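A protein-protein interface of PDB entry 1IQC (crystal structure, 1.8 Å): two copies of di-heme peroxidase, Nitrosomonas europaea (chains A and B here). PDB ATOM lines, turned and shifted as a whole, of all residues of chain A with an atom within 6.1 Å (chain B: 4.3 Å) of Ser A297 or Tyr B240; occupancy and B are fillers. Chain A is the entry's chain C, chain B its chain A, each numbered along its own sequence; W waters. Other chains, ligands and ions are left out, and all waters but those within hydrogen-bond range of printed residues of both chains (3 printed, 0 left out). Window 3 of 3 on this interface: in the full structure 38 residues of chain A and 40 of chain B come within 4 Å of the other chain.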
ATOM      1  N   ARG A  30      -5.998  24.159 -29.047  1.00  0.00           N
ATOM      2  CA  ARG A  30      -6.032  24.989 -27.846  1.00  0.00           C
ATOM      3  C   ARG A  30      -6.917  26.221 -28.005  1.00  0.00           C
ATOM      4  O   ARG A  30      -7.097  26.990 -27.058  1.00  0.00           O
ATOM      5  CB  ARG A  30      -4.616  25.382 -27.430  1.00  0.00           C
ATOM      6  CG  ARG A  30      -3.845  24.207 -26.861  1.00  0.00           C
ATOM      7  CD  ARG A  30      -2.369  24.488 -26.780  1.00  0.00           C
ATOM      8  NE  ARG A  30      -1.812  24.769 -28.100  1.00  0.00           N
ATOM      9  CZ  ARG A  30      -0.514  24.819 -28.358  1.00  0.00           C
ATOM     10  NH1 ARG A  30       0.360  24.601 -27.385  1.00  0.00           N
ATOM     11  NH2 ARG A  30      -0.088  25.093 -29.589  1.00  0.00           N
ATOM     12  N   VAL A 113      -4.187  32.416 -24.642  1.00  0.00           N
ATOM     13  CA  VAL A 113      -3.555  31.151 -24.975  1.00  0.00           C
ATOM     14  C   VAL A 113      -2.479  31.340 -26.032  1.00  0.00           C
ATOM     15  O   VAL A 113      -1.328  30.945 -25.839  1.00  0.00           O
ATOM     16  CB  VAL A 113      -4.602  30.144 -25.483  1.00  0.00           C
ATOM     17  CG1 VAL A 113      -3.924  28.903 -26.060  1.00  0.00           C
ATOM     18  CG2 VAL A 113      -5.527  29.771 -24.339  1.00  0.00           C
ATOM     19  N   SER A 116       0.538  33.496 -24.928  1.00  0.00           N
ATOM     20  CA  SER A 116       1.411  32.894 -23.922  1.00  0.00           C
ATOM     21  C   SER A 116       2.619  32.190 -24.537  1.00  0.00           C
ATOM     22  O   SER A 116       3.606  31.930 -23.850  1.00  0.00           O
ATOM     23  CB  SER A 116       0.624  31.887 -23.071  1.00  0.00           C
ATOM     24  OG  SER A 116       0.340  30.705 -23.808  1.00  0.00           O
ATOM     25  N   MET A 117       2.542  31.889 -25.829  1.00  0.00           N
ATOM     26  CA  MET A 117       3.622  31.188 -26.514  1.00  0.00           C
ATOM     27  C   MET A 117       4.511  32.096 -27.366  1.00  0.00           C
ATOM     28  O   MET A 117       4.061  32.677 -28.350  1.00  0.00           O
ATOM     29  CB  MET A 117       3.025  30.070 -27.375  1.00  0.00           C
ATOM     30  CG  MET A 117       2.330  28.995 -26.548  1.00  0.00           C
ATOM     31  SD  MET A 117       1.413  27.834 -27.559  1.00  0.00           S
ATOM     32  CE  MET A 117      -0.241  28.285 -27.214  1.00  0.00           C
ATOM     33  N   PRO A 295       3.757  25.219 -31.520  1.00  0.00           N
ATOM     34  CA  PRO A 295       4.603  25.451 -30.347  1.00  0.00           C
ATOM     35  C   PRO A 295       3.964  24.857 -29.096  1.00  0.00           C
ATOM     36  O   PRO A 295       2.741  24.768 -28.988  1.00  0.00           O
ATOM     37  CB  PRO A 295       4.721  26.974 -30.293  1.00  0.00           C
ATOM     38  CG  PRO A 295       3.430  27.441 -30.865  1.00  0.00           C
ATOM     39  CD  PRO A 295       3.178  26.480 -32.021  1.00  0.00           C
ATOM     40  N   PRO A 296       4.795  24.427 -28.135  1.00  0.00           N
ATOM     41  CA  PRO A 296       4.249  23.844 -26.912  1.00  0.00           C
ATOM     42  C   PRO A 296       3.689  24.877 -25.960  1.00  0.00           C
ATOM     43  O   PRO A 296       4.153  26.020 -25.918  1.00  0.00           O
ATOM     44  CB  PRO A 296       5.455  23.129 -26.307  1.00  0.00           C
ATOM     45  CG  PRO A 296       6.586  24.043 -26.685  1.00  0.00           C
ATOM     46  CD  PRO A 296       6.265  24.344 -28.145  1.00  0.00           C
ATOM     47  N   SER A 297       2.679  24.468 -25.205  1.00  0.00           N
ATOM     48  CA  SER A 297       2.103  25.336 -24.192  1.00  0.00           C
ATOM     49  C   SER A 297       3.207  25.421 -23.138  1.00  0.00           C
ATOM     50  O   SER A 297       4.095  24.564 -23.105  1.00  0.00           O
ATOM     51  CB  SER A 297       0.862  24.680 -23.577  1.00  0.00           C
ATOM     52  OG  SER A 297      -0.213  24.618 -24.504  1.00  0.00           O
ATOM     53  N   ASN A 298       3.177  26.449 -22.296  1.00  0.00           N
ATOM     54  CA  ASN A 298       4.183  26.574 -21.243  1.00  0.00           C
ATOM     55  C   ASN A 298       3.475  26.898 -19.924  1.00  0.00           C
ATOM     56  O   ASN A 298       2.252  26.953 -19.879  1.00  0.00           O
ATOM     57  CB  ASN A 298       5.225  27.641 -21.601  1.00  0.00           C
ATOM     58  CG  ASN A 298       4.606  28.976 -21.935  1.00  0.00           C
ATOM     59  OD1 ASN A 298       4.656  29.430 -23.079  1.00  0.00           O
ATOM     60  ND2 ASN A 298       4.016  29.612 -20.941  1.00  0.00           N
ATOM     61  N   ASN A 299       4.232  27.106 -18.853  1.00  0.00           N
ATOM     62  CA  ASN A 299       3.620  27.374 -17.556  1.00  0.00           C
ATOM     63  C   ASN A 299       2.668  28.566 -17.510  1.00  0.00           C
ATOM     64  O   ASN A 299       1.817  28.643 -16.624  1.00  0.00           O
ATOM     65  CB  ASN A 299       4.708  27.521 -16.481  1.00  0.00           C
ATOM     66  CG  ASN A 299       5.440  26.214 -16.220  1.00  0.00           C
ATOM     67  OD1 ASN A 299       5.090  25.171 -16.779  1.00  0.00           O
ATOM     68  ND2 ASN A 299       6.460  26.261 -15.362  1.00  0.00           N
ATOM     69  N   THR A 301       0.594  29.351 -20.083  1.00  0.00           N
ATOM     70  CA  THR A 301      -0.570  29.051 -20.915  1.00  0.00           C
ATOM     71  C   THR A 301      -1.793  28.581 -20.122  1.00  0.00           C
ATOM     72  O   THR A 301      -1.687  27.686 -19.283  1.00  0.00           O
ATOM     73  CB  THR A 301      -0.208  27.958 -21.956  1.00  0.00           C
ATOM     74  OG1 THR A 301       1.004  28.321 -22.629  1.00  0.00           O
ATOM     75  CG2 THR A 301      -1.322  27.796 -22.983  1.00  0.00           C
ATOM     76  N   PRO A 302      -2.969  29.194 -20.361  1.00  0.00           N
ATOM     77  CA  PRO A 302      -4.182  28.783 -19.645  1.00  0.00           C
ATOM     78  C   PRO A 302      -4.356  27.298 -19.933  1.00  0.00           C
ATOM     79  O   PRO A 302      -4.257  26.885 -21.085  1.00  0.00           O
ATOM     80  CB  PRO A 302      -5.267  29.631 -20.297  1.00  0.00           C
ATOM     81  CG  PRO A 302      -4.533  30.892 -20.636  1.00  0.00           C
ATOM     82  CD  PRO A 302      -3.234  30.376 -21.205  1.00  0.00           C
ATOM     83  N   MET B  47       1.508  18.319 -32.082  1.00  0.00           N
ATOM     84  CA  MET B  47       1.753  18.741 -30.699  1.00  0.00           C
ATOM     85  C   MET B  47       2.731  17.930 -29.839  1.00  0.00           C
ATOM     86  O   MET B  47       2.914  18.248 -28.663  1.00  0.00           O
ATOM     87  CB  MET B  47       0.411  18.782 -29.959  1.00  0.00           C
ATOM     88  CG  MET B  47      -0.618  19.740 -30.533  1.00  0.00           C
ATOM     89  SD  MET B  47      -0.341  21.408 -29.957  1.00  0.00           S
ATOM     90  CE  MET B  47      -0.816  21.233 -28.203  1.00  0.00           C
ATOM     91  N   ASN B  52      -2.293  16.087 -24.634  1.00  0.00           N
ATOM     92  CA  ASN B  52      -2.015  17.156 -23.689  1.00  0.00           C
ATOM     93  C   ASN B  52      -3.117  17.502 -22.702  1.00  0.00           C
ATOM     94  O   ASN B  52      -3.341  18.678 -22.395  1.00  0.00           O
ATOM     95  CB  ASN B  52      -1.588  18.402 -24.470  1.00  0.00           C
ATOM     96  CG  ASN B  52      -0.292  18.178 -25.234  1.00  0.00           C
ATOM     97  OD1 ASN B  52       0.790  18.070 -24.642  1.00  0.00           O
ATOM     98  ND2 ASN B  52      -0.395  18.083 -26.547  1.00  0.00           N
ATOM     99  N   ILE B 236       9.786  15.591 -23.639  1.00  0.00           N
ATOM    100  CA  ILE B 236       8.977  15.753 -22.432  1.00  0.00           C
ATOM    101  C   ILE B 236       8.397  17.166 -22.369  1.00  0.00           C
ATOM    102  O   ILE B 236       7.335  17.389 -21.794  1.00  0.00           O
ATOM    103  CB  ILE B 236       9.808  15.443 -21.160  1.00  0.00           C
ATOM    104  CG1 ILE B 236       8.886  15.326 -19.944  1.00  0.00           C
ATOM    105  CG2 ILE B 236      10.894  16.496 -20.958  1.00  0.00           C
ATOM    106  CD1 ILE B 236       7.925  14.147 -20.025  1.00  0.00           C
ATOM    107  N   GLU B 237       9.095  18.116 -22.987  1.00  0.00           N
ATOM    108  CA  GLU B 237       8.636  19.503 -23.031  1.00  0.00           C
ATOM    109  C   GLU B 237       7.290  19.628 -23.755  1.00  0.00           C
ATOM    110  O   GLU B 237       6.530  20.565 -23.514  1.00  0.00           O
ATOM    111  CB  GLU B 237       9.677  20.352 -23.771  1.00  0.00           C
ATOM    112  CG  GLU B 237       9.317  21.816 -23.968  1.00  0.00           C
ATOM    113  CD  GLU B 237      10.272  22.505 -24.929  1.00  0.00           C
ATOM    114  OE1 GLU B 237      10.386  23.746 -24.866  1.00  0.00           O
ATOM    115  OE2 GLU B 237      10.898  21.805 -25.751  1.00  0.00           O
ATOM    116  N   LEU B 238       6.988  18.679 -24.634  1.00  0.00           N
ATOM    117  CA  LEU B 238       5.755  18.733 -25.428  1.00  0.00           C
ATOM    118  C   LEU B 238       4.618  17.832 -24.981  1.00  0.00           C
ATOM    119  O   LEU B 238       3.551  17.857 -25.584  1.00  0.00           O
ATOM    120  CB  LEU B 238       6.057  18.357 -26.881  1.00  0.00           C
ATOM    121  CG  LEU B 238       7.347  18.862 -27.528  1.00  0.00           C
ATOM    122  CD1 LEU B 238       7.390  18.378 -28.968  1.00  0.00           C
ATOM    123  CD2 LEU B 238       7.400  20.371 -27.479  1.00  0.00           C
ATOM    124  N   THR B 239       4.831  17.061 -23.924  1.00  0.00           N
ATOM    125  CA  THR B 239       3.819  16.104 -23.511  1.00  0.00           C
ATOM    126  C   THR B 239       3.162  16.269 -22.142  1.00  0.00           C
ATOM    127  O   THR B 239       2.732  15.289 -21.536  1.00  0.00           O
ATOM    128  CB  THR B 239       4.405  14.692 -23.630  1.00  0.00           C
ATOM    129  OG1 THR B 239       5.490  14.555 -22.711  1.00  0.00           O
ATOM    130  CG2 THR B 239       4.945  14.472 -25.046  1.00  0.00           C
ATOM    131  N   TYR B 240       3.101  17.504 -21.660  1.00  0.00           N
ATOM    132  CA  TYR B 240       2.424  17.837 -20.401  1.00  0.00           C
ATOM    133  C   TYR B 240       0.941  17.460 -20.585  1.00  0.00           C
ATOM    134  O   TYR B 240       0.458  17.386 -21.717  1.00  0.00           O
ATOM    135  CB  TYR B 240       2.549  19.351 -20.170  1.00  0.00           C
ATOM    136  CG  TYR B 240       2.280  20.139 -21.435  1.00  0.00           C
ATOM    137  CD1 TYR B 240       0.972  20.434 -21.835  1.00  0.00           C
ATOM    138  CD2 TYR B 240       3.319  20.439 -22.321  1.00  0.00           C
ATOM    139  CE1 TYR B 240       0.706  20.988 -23.086  1.00  0.00           C
ATOM    140  CE2 TYR B 240       3.061  20.991 -23.578  1.00  0.00           C
ATOM    141  CZ  TYR B 240       1.755  21.256 -23.954  1.00  0.00           C
ATOM    142  OH  TYR B 240       1.494  21.750 -25.212  1.00  0.00           O
ATOM    143  N   PRO B 241       0.202  17.189 -19.486  1.00  0.00           N
ATOM    144  CA  PRO B 241       0.645  17.194 -18.087  1.00  0.00           C
ATOM    145  C   PRO B 241       1.440  15.921 -17.830  1.00  0.00           C
ATOM    146  O   PRO B 241       1.446  15.020 -18.673  1.00  0.00           O
ATOM    147  CB  PRO B 241      -0.669  17.253 -17.305  1.00  0.00           C
ATOM    148  CG  PRO B 241      -1.623  16.527 -18.192  1.00  0.00           C
ATOM    149  CD  PRO B 241      -1.267  17.076 -19.562  1.00  0.00           C
ATOM    150  N   TYR B 242       2.078  15.818 -16.671  1.00  0.00           N
ATOM    151  CA  TYR B 242       2.921  14.659 -16.402  1.00  0.00           C
ATOM    152  C   TYR B 242       2.432  13.578 -15.444  1.00  0.00           C
ATOM    153  O   TYR B 242       1.499  13.789 -14.670  1.00  0.00           O
ATOM    154  CB  TYR B 242       4.304  15.160 -16.002  1.00  0.00           C
ATOM    155  CG  TYR B 242       4.821  16.148 -17.020  1.00  0.00           C
ATOM    156  CD1 TYR B 242       4.749  17.524 -16.793  1.00  0.00           C
ATOM    157  CD2 TYR B 242       5.298  15.706 -18.256  1.00  0.00           C
ATOM    158  CE1 TYR B 242       5.135  18.436 -17.775  1.00  0.00           C
ATOM    159  CE2 TYR B 242       5.681  16.608 -19.242  1.00  0.00           C
ATOM    160  CZ  TYR B 242       5.598  17.967 -19.000  1.00  0.00           C
ATOM    161  OH  TYR B 242       5.972  18.850 -19.992  1.00  0.00           O
ATOM    162  N   ALA B 249       1.195  19.285 -13.520  1.00  0.00           N
ATOM    163  CA  ALA B 249       1.006  20.156 -14.675  1.00  0.00           C
ATOM    164  C   ALA B 249       2.286  20.741 -15.257  1.00  0.00           C
ATOM    165  O   ALA B 249       2.346  21.031 -16.449  1.00  0.00           O
ATOM    166  CB  ALA B 249       0.033  21.289 -14.322  1.00  0.00           C
HETATM  167  O   HOH W   1       3.148  21.675 -29.512  1.00  0.00           O
HETATM  168  O   HOH W   2       6.001  22.849 -22.174  1.00  0.00           O
HETATM  169  O   HOH W   3       3.287  23.536 -18.547  1.00  0.00           O
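The side-chain sulfur of Met B47 sits at hydrogen-bond distance from the guanidinium group of Arg A30 (3.7 Å).
The backbone NH (N) of Ser A297 is in hydrogen-bond range of the side-chain hydroxyl (OH) of Tyr B240, at 3.0 Å.
The side-chain amide oxygen of Asn B52 lies close to the backbone carbonyl oxygen of Leu B238 (2.9 Å).
The side-chain amide oxygen of Asn B52 lies close to the backbone carbonyl oxygen of Tyr B240, 3.0 Å away.
The guanidinium group of Arg A30 is in hydrogen-bond range of the side-chain sulfur of Met A117.
The guanidinium group of Arg A30 sits at hydrogen-bond distance from the backbone carbonyl oxygen of Pro A295.
OG of Ser A297 lies within hydrogen-bond range of NH1 of Arg A30 (2.9 Å).
Arg A30 touches Tyr B240 (NH1 to OH, 3.8 Å).
Glu B237 touches Pro A296.
Pro A296 touches Leu B238 (CB to CD2, 3.6 Å).
Pro A296 touches Tyr B240 (CA to OH, 3.9 Å).
Printed residues of chain B within 4 Å of Pro A296: Glu B237 (3.9 Å), Leu B238 (3.6 Å) and Tyr B240 (3.9 Å).
Of the printed residues of chain A, Met B47 touches Arg A30.
Of chain A, only Arg A30, Pro A296 and Ser A297 come within 4 Å of Tyr B240.
The nearest printed residue of chain A that does not touch Met B47 is Pro A295 (4.7 Å).
Hydrophobic or aromatic side chains of chain B within 4 Å of the printed part of chain A: Met B47, Leu B238 and Tyr B240.
Along chain A the printed residues that touch a printed residue of chain B span positions 30 to 297.
Among the printed residues, 6 pairs touch across the chains.
Among the printed residues, no Asp or Glu carboxylate lies within 4 Å of a Lys or Arg side-chain nitrogen of the other chain.
No position is printed for both chains.
Water W2 lies within hydrogen-bond range of O of Glu B237 and O of Ser A297.
Water W3 bridges OD1 of Asn A299 (3.0 Å) and O of Ala B249 (3.4 Å).
Water W1 bridges the backbone carbonyl oxygen (O) of Pro A295 and the side-chain sulfur (SD) of Met B47.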
